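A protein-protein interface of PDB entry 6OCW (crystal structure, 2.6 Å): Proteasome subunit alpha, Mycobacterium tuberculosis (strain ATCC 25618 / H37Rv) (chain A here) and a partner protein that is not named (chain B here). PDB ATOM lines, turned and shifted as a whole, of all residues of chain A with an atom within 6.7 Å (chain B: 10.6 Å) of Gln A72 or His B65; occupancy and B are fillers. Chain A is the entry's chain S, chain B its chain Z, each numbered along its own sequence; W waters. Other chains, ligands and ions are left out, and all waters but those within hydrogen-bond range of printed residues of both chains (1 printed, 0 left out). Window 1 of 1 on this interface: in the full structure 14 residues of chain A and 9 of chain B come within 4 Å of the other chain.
Among the printed residues, pairs that only touch across the chains: Ile A71 with Lys B68 (3.3 Å), Arg A68 with Leu B69 (3.7 Å), Ile A71 with His B65 (3.8 Å) and Ile A71 with Leu B69 (3.99 Å).
NH1 of Arg A67 lies within hydrogen-bond range of O of Lys B68 (2.9 Å).
The guanidinium group (NH2) of Arg A67 lies within hydrogen-bond range of the backbone carbonyl oxygen (O) of Leu B69 (2.7 Å).
The side-chain carboxylate of Glu B70 lies within salt-bridge range of the guanidinium group of Arg A68.
A ring nitrogen (NE2) of His B65 sits close to the side-chain amide oxygen (OE1) of Gln A72 (3.4 Å).
OD1 of Asp A75 lies within salt-bridge range of NZ of Lys B68, 2.4 Å away.
A ring nitrogen (ND1) of His B65 lies close to the side-chain carboxylate (OD2) of Asp A75 (2.4 Å).
Of chain B, only His B65 (3.3 Å) comes within 4 Å of Gln A72.
Of chain A, only Ile A71, Gln A72 and Asp A75 come within 4 Å of His B65.
No residue of chain B comes within 4 Å of Gly A69.
No residue of chain B comes within 4 Å of Gly A70.
No residue of chain B comes within 4 Å of Ala A74.
Of chain B, only His B65 (2.4 Å) and Lys B68 (2.4 Å) come within 4 Å of Asp A75.
No residue of chain B comes within 4 Å of Thr A76.
Of the printed residues of chain B, Arg A68 touches Leu B69 (3.7 Å) and Glu B70 (2.8 Å).
Of the printed residues of chain A, Glu B70 touches Arg A68 (2.8 Å).
Tyr B66 touches none of the printed residues of chain A.
The nearest residue of chain B that does not touch Gln A72 is Leu B69 (5.3 Å).
Water W1 bridges the side-chain carboxylate (OE1) of Glu B70 (2.7 Å) and the guanidinium group (NH2) of Arg A68 (2.8 Å).
Of the 23 printed residues of chain B, 4 touch a printed residue of chain A.
Hydrophobic or aromatic side chains of chain B that line the printed part of chain A: His B65 and Leu B69.
Printed residues of chain A that touch a printed residue of chain B: Arg A67, Arg A68, Ile A71, Gln A72 and Asp A75.
Among the printed residues, 10 pairs touch across the chains.
The side-chain hydroxyl (OG1) of Thr A76 is in hydrogen-bond range of the backbone carbonyl oxygen (O) of Gln A72 (3.0 Å).
OE2 of Glu B64 lies within salt-bridge range of NZ of Lys B68, 3.5 Å away.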
ATOM      1  N   ARG A  67     -15.281  23.081  19.944  1.00  0.00           N
ATOM      2  CA  ARG A  67     -14.794  21.721  20.099  1.00  0.00           C
ATOM      3  C   ARG A  67     -13.457  21.709  20.829  1.00  0.00           C
ATOM      4  O   ARG A  67     -13.249  20.933  21.769  1.00  0.00           O
ATOM      5  CB  ARG A  67     -14.676  21.083  18.715  1.00  0.00           C
ATOM      6  CG  ARG A  67     -14.159  19.660  18.685  1.00  0.00           C
ATOM      7  CD  ARG A  67     -13.883  19.271  17.258  1.00  0.00           C
ATOM      8  NE  ARG A  67     -12.689  19.930  16.754  1.00  0.00           N
ATOM      9  CZ  ARG A  67     -11.477  19.387  16.857  1.00  0.00           C
ATOM     10  NH1 ARG A  67     -11.346  18.199  17.447  1.00  0.00           N
ATOM     11  NH2 ARG A  67     -10.401  20.013  16.384  1.00  0.00           N
ATOM     12  N   ARG A  68     -12.540  22.584  20.406  1.00  0.00           N
ATOM     13  CA  ARG A  68     -11.224  22.653  21.026  1.00  0.00           C
ATOM     14  C   ARG A  68     -11.326  23.082  22.476  1.00  0.00           C
ATOM     15  O   ARG A  68     -10.625  22.545  23.343  1.00  0.00           O
ATOM     16  CB  ARG A  68     -10.338  23.611  20.245  1.00  0.00           C
ATOM     17  CG  ARG A  68     -10.095  23.146  18.833  1.00  0.00           C
ATOM     18  CD  ARG A  68      -9.125  24.032  18.110  1.00  0.00           C
ATOM     19  NE  ARG A  68      -8.834  23.454  16.810  1.00  0.00           N
ATOM     20  CZ  ARG A  68      -7.704  22.820  16.519  1.00  0.00           C
ATOM     21  NH1 ARG A  68      -6.755  22.709  17.444  1.00  0.00           N
ATOM     22  NH2 ARG A  68      -7.525  22.312  15.305  1.00  0.00           N
ATOM     23  N   GLY A  69     -12.205  24.039  22.768  1.00  0.00           N
ATOM     24  CA  GLY A  69     -12.394  24.436  24.149  1.00  0.00           C
ATOM     25  C   GLY A  69     -12.889  23.280  24.992  1.00  0.00           C
ATOM     26  O   GLY A  69     -12.497  23.129  26.157  1.00  0.00           O
ATOM     27  N   GLY A  70     -13.740  22.436  24.403  1.00  0.00           N
ATOM     28  CA  GLY A  70     -14.294  21.325  25.145  1.00  0.00           C
ATOM     29  C   GLY A  70     -13.257  20.262  25.424  1.00  0.00           C
ATOM     30  O   GLY A  70     -13.211  19.693  26.519  1.00  0.00           O
ATOM     31  N   ILE A  71     -12.406  19.980  24.441  1.00  0.00           N
ATOM     32  CA  ILE A  71     -11.326  19.038  24.679  1.00  0.00           C
ATOM     33  C   ILE A  71     -10.397  19.570  25.770  1.00  0.00           C
ATOM     34  O   ILE A  71      -9.969  18.828  26.668  1.00  0.00           O
ATOM     35  CB  ILE A  71     -10.600  18.763  23.355  1.00  0.00           C
ATOM     36  CG1 ILE A  71     -11.588  18.091  22.384  1.00  0.00           C
ATOM     37  CG2 ILE A  71      -9.317  17.962  23.595  1.00  0.00           C
ATOM     38  CD1 ILE A  71     -11.095  17.962  20.947  1.00  0.00           C
ATOM     39  N   GLN A  72     -10.107  20.876  25.730  1.00  0.00           N
ATOM     40  CA  GLN A  72      -9.335  21.508  26.798  1.00  0.00           C
ATOM     41  C   GLN A  72      -9.986  21.264  28.156  1.00  0.00           C
ATOM     42  O   GLN A  72      -9.331  20.820  29.113  1.00  0.00           O
ATOM     43  CB  GLN A  72      -9.207  23.006  26.511  1.00  0.00           C
ATOM     44  CG  GLN A  72      -8.440  23.820  27.554  1.00  0.00           C
ATOM     45  CD  GLN A  72      -6.995  23.355  27.755  1.00  0.00           C
ATOM     46  OE1 GLN A  72      -6.582  22.318  27.236  1.00  0.00           O
ATOM     47  NE2 GLN A  72      -6.222  24.131  28.514  1.00  0.00           N
ATOM     48  N   PHE A  73     -11.287  21.529  28.255  1.00  0.00           N
ATOM     49  CA  PHE A  73     -11.975  21.397  29.533  1.00  0.00           C
ATOM     50  C   PHE A  73     -11.974  19.956  30.032  1.00  0.00           C
ATOM     51  O   PHE A  73     -11.794  19.705  31.229  1.00  0.00           O
ATOM     52  CB  PHE A  73     -13.397  21.913  29.384  1.00  0.00           C
ATOM     53  CG  PHE A  73     -14.261  21.675  30.580  1.00  0.00           C
ATOM     54  CD1 PHE A  73     -15.003  20.512  30.697  1.00  0.00           C
ATOM     55  CD2 PHE A  73     -14.372  22.640  31.570  1.00  0.00           C
ATOM     56  CE1 PHE A  73     -15.815  20.308  31.790  1.00  0.00           C
ATOM     57  CE2 PHE A  73     -15.190  22.440  32.670  1.00  0.00           C
ATOM     58  CZ  PHE A  73     -15.909  21.280  32.782  1.00  0.00           C
ATOM     59  N   ALA A  74     -12.191  18.996  29.135  1.00  0.00           N
ATOM     60  CA  ALA A  74     -12.311  17.612  29.566  1.00  0.00           C
ATOM     61  C   ALA A  74     -10.957  17.053  29.975  1.00  0.00           C
ATOM     62  O   ALA A  74     -10.838  16.405  31.019  1.00  0.00           O
ATOM     63  CB  ALA A  74     -12.946  16.764  28.463  1.00  0.00           C
ATOM     64  N   ASP A  75      -9.920  17.293  29.167  1.00  0.00           N
ATOM     65  CA  ASP A  75      -8.597  16.801  29.543  1.00  0.00           C
ATOM     66  C   ASP A  75      -8.130  17.450  30.849  1.00  0.00           C
ATOM     67  O   ASP A  75      -7.499  16.790  31.690  1.00  0.00           O
ATOM     68  CB  ASP A  75      -7.584  17.051  28.414  1.00  0.00           C
ATOM     69  CG  ASP A  75      -7.881  16.259  27.128  1.00  0.00           C
ATOM     70  OD1 ASP A  75      -8.595  15.239  27.168  1.00  0.00           O
ATOM     71  OD2 ASP A  75      -7.359  16.648  26.064  1.00  0.00           O
ATOM     72  N   THR A  76      -8.475  18.731  31.054  1.00  0.00           N
ATOM     73  CA  THR A  76      -8.107  19.430  32.287  1.00  0.00           C
ATOM     74  C   THR A  76      -8.841  18.869  33.509  1.00  0.00           C
ATOM     75  O   THR A  76      -8.233  18.633  34.558  1.00  0.00           O
ATOM     76  CB  THR A  76      -8.378  20.932  32.146  1.00  0.00           C
ATOM     77  OG1 THR A  76      -7.379  21.538  31.309  1.00  0.00           O
ATOM     78  CG2 THR A  76      -8.358  21.602  33.504  1.00  0.00           C
ATOM     79  N   ARG A  77     -10.149  18.658  33.411  1.00  0.00           N
ATOM     80  CA  ARG A  77     -10.845  18.073  34.552  1.00  0.00           C
ATOM     81  C   ARG A  77     -10.341  16.664  34.836  1.00  0.00           C
ATOM     82  O   ARG A  77     -10.027  16.325  35.983  1.00  0.00           O
ATOM     83  CB  ARG A  77     -12.351  18.070  34.316  1.00  0.00           C
ATOM     84  CG  ARG A  77     -12.982  19.429  34.523  1.00  0.00           C
ATOM     85  CD  ARG A  77     -12.789  19.976  35.946  1.00  0.00           C
ATOM     86  NE  ARG A  77     -13.716  21.084  36.144  1.00  0.00           N
ATOM     87  CZ  ARG A  77     -15.020  20.931  36.367  1.00  0.00           C
ATOM     88  NH1 ARG A  77     -15.537  19.708  36.436  1.00  0.00           N
ATOM     89  NH2 ARG A  77     -15.808  21.995  36.527  1.00  0.00           N
ATOM     90  N   THR B  37       1.540   4.631  27.633  1.00  0.00           N
ATOM     91  CA  THR B  37       1.186   6.032  27.493  1.00  0.00           C
ATOM     92  C   THR B  37       0.358   6.310  26.240  1.00  0.00           C
ATOM     93  O   THR B  37      -0.336   7.331  26.197  1.00  0.00           O
ATOM     94  CB  THR B  37       2.454   6.886  27.550  1.00  0.00           C
ATOM     95  OG1 THR B  37       3.490   6.250  26.802  1.00  0.00           O
ATOM     96  CG2 THR B  37       2.923   6.995  29.000  1.00  0.00           C
ATOM     97  N   ASP B  38       0.362   5.421  25.248  1.00  0.00           N
ATOM     98  CA  ASP B  38      -0.680   5.471  24.214  1.00  0.00           C
ATOM     99  C   ASP B  38      -0.656   4.152  23.445  1.00  0.00           C
ATOM    100  O   ASP B  38       0.113   3.239  23.764  1.00  0.00           O
ATOM    101  CB  ASP B  38      -0.550   6.707  23.296  1.00  0.00           C
ATOM    102  CG  ASP B  38       0.551   6.579  22.232  1.00  0.00           C
ATOM    103  OD1 ASP B  38       1.224   5.521  22.139  1.00  0.00           O
ATOM    104  OD2 ASP B  38       0.753   7.565  21.482  1.00  0.00           O
ATOM    105  N   ARG B  57       1.484  10.306  33.820  1.00  0.00           N
ATOM    106  CA  ARG B  57       0.083  10.679  33.676  1.00  0.00           C
ATOM    107  C   ARG B  57      -0.065  11.892  32.761  1.00  0.00           C
ATOM    108  O   ARG B  57      -0.773  11.840  31.745  1.00  0.00           O
ATOM    109  CB  ARG B  57      -0.514  10.935  35.063  1.00  0.00           C
ATOM    110  CG  ARG B  57      -2.014  10.989  35.080  1.00  0.00           C
ATOM    111  CD  ARG B  57      -2.597  10.795  36.469  1.00  0.00           C
ATOM    112  NE  ARG B  57      -4.042  10.992  36.426  1.00  0.00           N
ATOM    113  CZ  ARG B  57      -4.658  12.128  36.751  1.00  0.00           C
ATOM    114  NH1 ARG B  57      -3.955  13.169  37.181  1.00  0.00           N
ATOM    115  NH2 ARG B  57      -5.983  12.222  36.654  1.00  0.00           N
ATOM    116  N   LEU B  58       0.635  12.986  33.087  1.00  0.00           N
ATOM    117  CA  LEU B  58       0.562  14.198  32.272  1.00  0.00           C
ATOM    118  C   LEU B  58       1.044  13.960  30.848  1.00  0.00           C
ATOM    119  O   LEU B  58       0.516  14.565  29.913  1.00  0.00           O
ATOM    120  CB  LEU B  58       1.387  15.300  32.933  1.00  0.00           C
ATOM    121  CG  LEU B  58       1.444  16.702  32.355  1.00  0.00           C
ATOM    122  CD1 LEU B  58       0.042  17.215  32.140  1.00  0.00           C
ATOM    123  CD2 LEU B  58       2.166  17.571  33.342  1.00  0.00           C
ATOM    124  N   TYR B  59       2.043  13.091  30.666  1.00  0.00           N
ATOM    125  CA  TYR B  59       2.563  12.803  29.333  1.00  0.00           C
ATOM    126  C   TYR B  59       1.510  12.126  28.466  1.00  0.00           C
ATOM    127  O   TYR B  59       1.267  12.538  27.317  1.00  0.00           O
ATOM    128  CB  TYR B  59       3.816  11.930  29.440  1.00  0.00           C
ATOM    129  CG  TYR B  59       4.519  11.673  28.118  1.00  0.00           C
ATOM    130  CD1 TYR B  59       4.824  12.722  27.260  1.00  0.00           C
ATOM    131  CD2 TYR B  59       4.891  10.378  27.737  1.00  0.00           C
ATOM    132  CE1 TYR B  59       5.468  12.496  26.047  1.00  0.00           C
ATOM    133  CE2 TYR B  59       5.539  10.137  26.532  1.00  0.00           C
ATOM    134  CZ  TYR B  59       5.827  11.202  25.691  1.00  0.00           C
ATOM    135  OH  TYR B  59       6.472  10.985  24.492  1.00  0.00           O
ATOM    136  N   ALA B  60       0.875  11.076  28.994  1.00  0.00           N
ATOM    137  CA  ALA B  60      -0.157  10.416  28.203  1.00  0.00           C
ATOM    138  C   ALA B  60      -1.305  11.378  27.910  1.00  0.00           C
ATOM    139  O   ALA B  60      -1.829  11.407  26.786  1.00  0.00           O
ATOM    140  CB  ALA B  60      -0.647   9.150  28.907  1.00  0.00           C
ATOM    141  N   VAL B  61      -1.680  12.204  28.895  1.00  0.00           N
ATOM    142  CA  VAL B  61      -2.732  13.189  28.653  1.00  0.00           C
ATOM    143  C   VAL B  61      -2.324  14.166  27.553  1.00  0.00           C
ATOM    144  O   VAL B  61      -3.164  14.603  26.757  1.00  0.00           O
ATOM    145  CB  VAL B  61      -3.098  13.934  29.949  1.00  0.00           C
ATOM    146  CG1 VAL B  61      -3.766  15.267  29.622  1.00  0.00           C
ATOM    147  CG2 VAL B  61      -4.011  13.081  30.789  1.00  0.00           C
ATOM    148  N   GLU B  62      -1.042  14.547  27.498  1.00  0.00           N
ATOM    149  CA  GLU B  62      -0.602  15.474  26.453  1.00  0.00           C
ATOM    150  C   GLU B  62      -0.718  14.837  25.069  1.00  0.00           C
ATOM    151  O   GLU B  62      -1.261  15.449  24.133  1.00  0.00           O
ATOM    152  CB  GLU B  62       0.828  15.945  26.716  1.00  0.00           C
ATOM    153  CG  GLU B  62       1.351  16.845  25.621  1.00  0.00           C
ATOM    154  CD  GLU B  62       2.705  17.488  25.916  1.00  0.00           C
ATOM    155  OE1 GLU B  62       3.354  17.125  26.924  1.00  0.00           O
ATOM    156  OE2 GLU B  62       3.122  18.367  25.118  1.00  0.00           O
ATOM    157  N   LEU B  63      -0.235  13.594  24.929  1.00  0.00           N
ATOM    158  CA  LEU B  63      -0.330  12.906  23.641  1.00  0.00           C
ATOM    159  C   LEU B  63      -1.787  12.770  23.177  1.00  0.00           C
ATOM    160  O   LEU B  63      -2.115  13.029  22.004  1.00  0.00           O
ATOM    161  CB  LEU B  63       0.351  11.533  23.738  1.00  0.00           C
ATOM    162  CG  LEU B  63       1.870  11.501  23.949  1.00  0.00           C
ATOM    163  CD1 LEU B  63       2.407  10.083  23.906  1.00  0.00           C
ATOM    164  CD2 LEU B  63       2.581  12.344  22.918  1.00  0.00           C
ATOM    165  N   GLU B  64      -2.677  12.334  24.077  1.00  0.00           N
ATOM    166  CA  GLU B  64      -4.072  12.190  23.677  1.00  0.00           C
ATOM    167  C   GLU B  64      -4.700  13.546  23.382  1.00  0.00           C
ATOM    168  O   GLU B  64      -5.544  13.675  22.482  1.00  0.00           O
ATOM    169  CB  GLU B  64      -4.858  11.458  24.765  1.00  0.00           C
ATOM    170  CG  GLU B  64      -6.222  11.005  24.295  1.00  0.00           C
ATOM    171  CD  GLU B  64      -7.005  10.269  25.366  1.00  0.00           C
ATOM    172  OE1 GLU B  64      -6.836   9.028  25.492  1.00  0.00           O
ATOM    173  OE2 GLU B  64      -7.784  10.940  26.080  1.00  0.00           O
ATOM    174  N   HIS B  65      -4.299  14.567  24.127  1.00  0.00           N
ATOM    175  CA  HIS B  65      -4.790  15.905  23.861  1.00  0.00           C
ATOM    176  C   HIS B  65      -4.481  16.311  22.426  1.00  0.00           C
ATOM    177  O   HIS B  65      -5.375  16.731  21.680  1.00  0.00           O
ATOM    178  CB  HIS B  65      -4.168  16.869  24.866  1.00  0.00           C
ATOM    179  CG  HIS B  65      -4.782  18.229  24.868  1.00  0.00           C
ATOM    180  ND1 HIS B  65      -6.043  18.471  25.360  1.00  0.00           N
ATOM    181  CD2 HIS B  65      -4.294  19.428  24.470  1.00  0.00           C
ATOM    182  CE1 HIS B  65      -6.315  19.760  25.248  1.00  0.00           C
ATOM    183  NE2 HIS B  65      -5.266  20.365  24.718  1.00  0.00           N
ATOM    184  N   TYR B  66      -3.221  16.164  22.006  1.00  0.00           N
ATOM    185  CA  TYR B  66      -2.907  16.472  20.614  1.00  0.00           C
ATOM    186  C   TYR B  66      -3.760  15.641  19.657  1.00  0.00           C
ATOM    187  O   TYR B  66      -4.317  16.172  18.687  1.00  0.00           O
ATOM    188  CB  TYR B  66      -1.426  16.256  20.331  1.00  0.00           C
ATOM    189  CG  TYR B  66      -1.005  16.787  18.976  1.00  0.00           C
ATOM    190  CD1 TYR B  66      -1.233  16.056  17.811  1.00  0.00           C
ATOM    191  CD2 TYR B  66      -0.372  18.015  18.855  1.00  0.00           C
ATOM    192  CE1 TYR B  66      -0.841  16.546  16.566  1.00  0.00           C
ATOM    193  CE2 TYR B  66       0.021  18.512  17.614  1.00  0.00           C
ATOM    194  CZ  TYR B  66      -0.213  17.778  16.479  1.00  0.00           C
ATOM    195  OH  TYR B  66       0.184  18.278  15.252  1.00  0.00           O
ATOM    196  N   GLU B  67      -3.898  14.338  19.927  1.00  0.00           N
ATOM    197  CA  GLU B  67      -4.664  13.483  19.022  1.00  0.00           C
ATOM    198  C   GLU B  67      -6.094  13.997  18.840  1.00  0.00           C
ATOM    199  O   GLU B  67      -6.575  14.125  17.709  1.00  0.00           O
ATOM    200  CB  GLU B  67      -4.656  12.037  19.533  1.00  0.00           C
ATOM    201  CG  GLU B  67      -5.427  11.043  18.670  1.00  0.00           C
ATOM    202  CD  GLU B  67      -5.214   9.582  19.078  1.00  0.00           C
ATOM    203  OE1 GLU B  67      -4.877   9.307  20.253  1.00  0.00           O
ATOM    204  OE2 GLU B  67      -5.376   8.700  18.207  1.00  0.00           O
ATOM    205  N   LYS B  68      -6.793  14.300  19.940  1.00  0.00           N
ATOM    206  CA  LYS B  68      -8.180  14.735  19.804  1.00  0.00           C
ATOM    207  C   LYS B  68      -8.282  16.156  19.255  1.00  0.00           C
ATOM    208  O   LYS B  68      -9.268  16.497  18.597  1.00  0.00           O
ATOM    209  CB  LYS B  68      -8.899  14.629  21.146  1.00  0.00           C
ATOM    210  CG  LYS B  68      -8.834  13.247  21.780  1.00  0.00           C
ATOM    211  CD  LYS B  68      -9.664  13.178  23.061  1.00  0.00           C
ATOM    212  CE  LYS B  68      -9.174  14.171  24.106  1.00  0.00           C
ATOM    213  NZ  LYS B  68      -9.679  13.862  25.480  1.00  0.00           N
ATOM    214  N   LEU B  69      -7.280  16.999  19.491  1.00  0.00           N
ATOM    215  CA  LEU B  69      -7.336  18.339  18.925  1.00  0.00           C
ATOM    216  C   LEU B  69      -7.161  18.306  17.414  1.00  0.00           C
ATOM    217  O   LEU B  69      -7.972  18.871  16.673  1.00  0.00           O
ATOM    218  CB  LEU B  69      -6.280  19.231  19.569  1.00  0.00           C
ATOM    219  CG  LEU B  69      -6.683  19.824  20.920  1.00  0.00           C
ATOM    220  CD1 LEU B  69      -5.552  20.721  21.445  1.00  0.00           C
ATOM    221  CD2 LEU B  69      -8.053  20.562  20.841  1.00  0.00           C
ATOM    222  N   GLU B  70      -6.111  17.652  16.937  1.00  0.00           N
ATOM    223  CA  GLU B  70      -5.732  17.711  15.536  1.00  0.00           C
ATOM    224  C   GLU B  70      -6.288  16.568  14.697  1.00  0.00           C
ATOM    225  O   GLU B  70      -6.174  16.609  13.466  1.00  0.00           O
ATOM    226  CB  GLU B  70      -4.208  17.737  15.428  1.00  0.00           C
ATOM    227  CG  GLU B  70      -3.625  18.822  16.284  1.00  0.00           C
ATOM    228  CD  GLU B  70      -4.129  20.174  15.860  1.00  0.00           C
ATOM    229  OE1 GLU B  70      -3.904  20.514  14.674  1.00  0.00           O
ATOM    230  OE2 GLU B  70      -4.763  20.877  16.686  1.00  0.00           O
ATOM    231  N   GLY B  71      -6.891  15.560  15.316  1.00  0.00           N
ATOM    232  CA  GLY B  71      -7.421  14.451  14.561  1.00  0.00           C
ATOM    233  C   GLY B  71      -6.407  13.397  14.191  1.00  0.00           C
ATOM    234  O   GLY B  71      -6.778  12.396  13.569  1.00  0.00           O
ATOM    235  N   VAL B  72      -5.146  13.568  14.562  1.00  0.00           N
ATOM    236  CA  VAL B  72      -4.139  12.579  14.194  1.00  0.00           C
ATOM    237  C   VAL B  72      -3.094  12.547  15.300  1.00  0.00           C
ATOM    238  O   VAL B  72      -2.859  13.573  15.951  1.00  0.00           O
ATOM    239  CB  VAL B  72      -3.526  12.895  12.822  1.00  0.00           C
ATOM    240  CG1 VAL B  72      -2.551  14.076  12.919  1.00  0.00           C
ATOM    241  CG2 VAL B  72      -2.871  11.668  12.254  1.00  0.00           C
ATOM    242  N   PRO B  73      -2.473  11.406  15.577  1.00  0.00           N
ATOM    243  CA  PRO B  73      -1.494  11.358  16.667  1.00  0.00           C
ATOM    244  C   PRO B  73      -0.199  12.046  16.272  1.00  0.00           C
ATOM    245  O   PRO B  73       0.113  12.210  15.092  1.00  0.00           O
ATOM    246  CB  PRO B  73      -1.283   9.857  16.908  1.00  0.00           C
ATOM    247  CG  PRO B  73      -1.712   9.192  15.660  1.00  0.00           C
ATOM    248  CD  PRO B  73      -2.727  10.083  14.984  1.00  0.00           C
ATOM    249  N   LEU B  74       0.545  12.481  17.287  1.00  0.00           N
ATOM    250  CA  LEU B  74       1.893  12.996  17.061  1.00  0.00           C
ATOM    251  C   LEU B  74       2.794  11.928  16.434  1.00  0.00           C
ATOM    252  O   LEU B  74       2.725  10.744  16.781  1.00  0.00           O
ATOM    253  CB  LEU B  74       2.500  13.473  18.386  1.00  0.00           C
ATOM    254  CG  LEU B  74       2.167  14.879  18.905  1.00  0.00           C
ATOM    255  CD1 LEU B  74       2.654  15.051  20.335  1.00  0.00           C
ATOM    256  CD2 LEU B  74       2.777  15.952  18.004  1.00  0.00           C
ATOM    257  N   LYS B  79       6.526  12.853  19.809  1.00  0.00           N
ATOM    258  CA  LYS B  79       6.396  12.327  21.162  1.00  0.00           C
ATOM    259  C   LYS B  79       7.720  12.443  21.908  1.00  0.00           C
ATOM    260  O   LYS B  79       7.755  12.801  23.100  1.00  0.00           O
ATOM    261  CB  LYS B  79       5.931  10.872  21.109  1.00  0.00           C
ATOM    262  CG  LYS B  79       4.677  10.626  20.273  1.00  0.00           C
ATOM    263  CD  LYS B  79       4.280   9.142  20.305  1.00  0.00           C
ATOM    264  CE  LYS B  79       3.038   8.877  19.477  1.00  0.00           C
ATOM    265  NZ  LYS B  79       2.689   7.430  19.437  1.00  0.00           N
ATOM    266  N   ARG B  82       8.274  16.076  22.923  1.00  0.00           N
ATOM    267  CA  ARG B  82       7.450  16.510  24.049  1.00  0.00           C
ATOM    268  C   ARG B  82       7.944  15.928  25.374  1.00  0.00           C
ATOM    269  O   ARG B  82       8.027  16.648  26.381  1.00  0.00           O
ATOM    270  CB  ARG B  82       5.983  16.156  23.791  1.00  0.00           C
ATOM    271  CG  ARG B  82       5.415  16.821  22.527  1.00  0.00           C
ATOM    272  CD  ARG B  82       5.824  18.271  22.421  1.00  0.00           C
ATOM    273  NE  ARG B  82       5.352  19.039  23.562  1.00  0.00           N
ATOM    274  CZ  ARG B  82       5.578  20.342  23.735  1.00  0.00           C
ATOM    275  NH1 ARG B  82       5.111  20.965  24.809  1.00  0.00           N
ATOM    276  NH2 ARG B  82       6.275  21.027  22.836  1.00  0.00           N
ATOM    277  N   MET B  86       9.418  18.094  28.644  1.00  0.00           N
ATOM    278  CA  MET B  86       8.964  17.940  30.019  1.00  0.00           C
ATOM    279  C   MET B  86      10.151  17.753  30.972  1.00  0.00           C
ATOM    280  O   MET B  86      10.211  18.379  32.045  1.00  0.00           O
ATOM    281  CB  MET B  86       7.983  16.768  30.075  1.00  0.00           C
ATOM    282  CG  MET B  86       6.989  16.790  31.201  1.00  0.00           C
ATOM    283  SD  MET B  86       5.758  15.469  31.081  1.00  0.00           S
ATOM    284  CE  MET B  86       5.054  15.846  29.485  1.00  0.00           C
HETATM  285  O   HOH W   1      -5.733  21.810  13.179  1.00  0.00           O
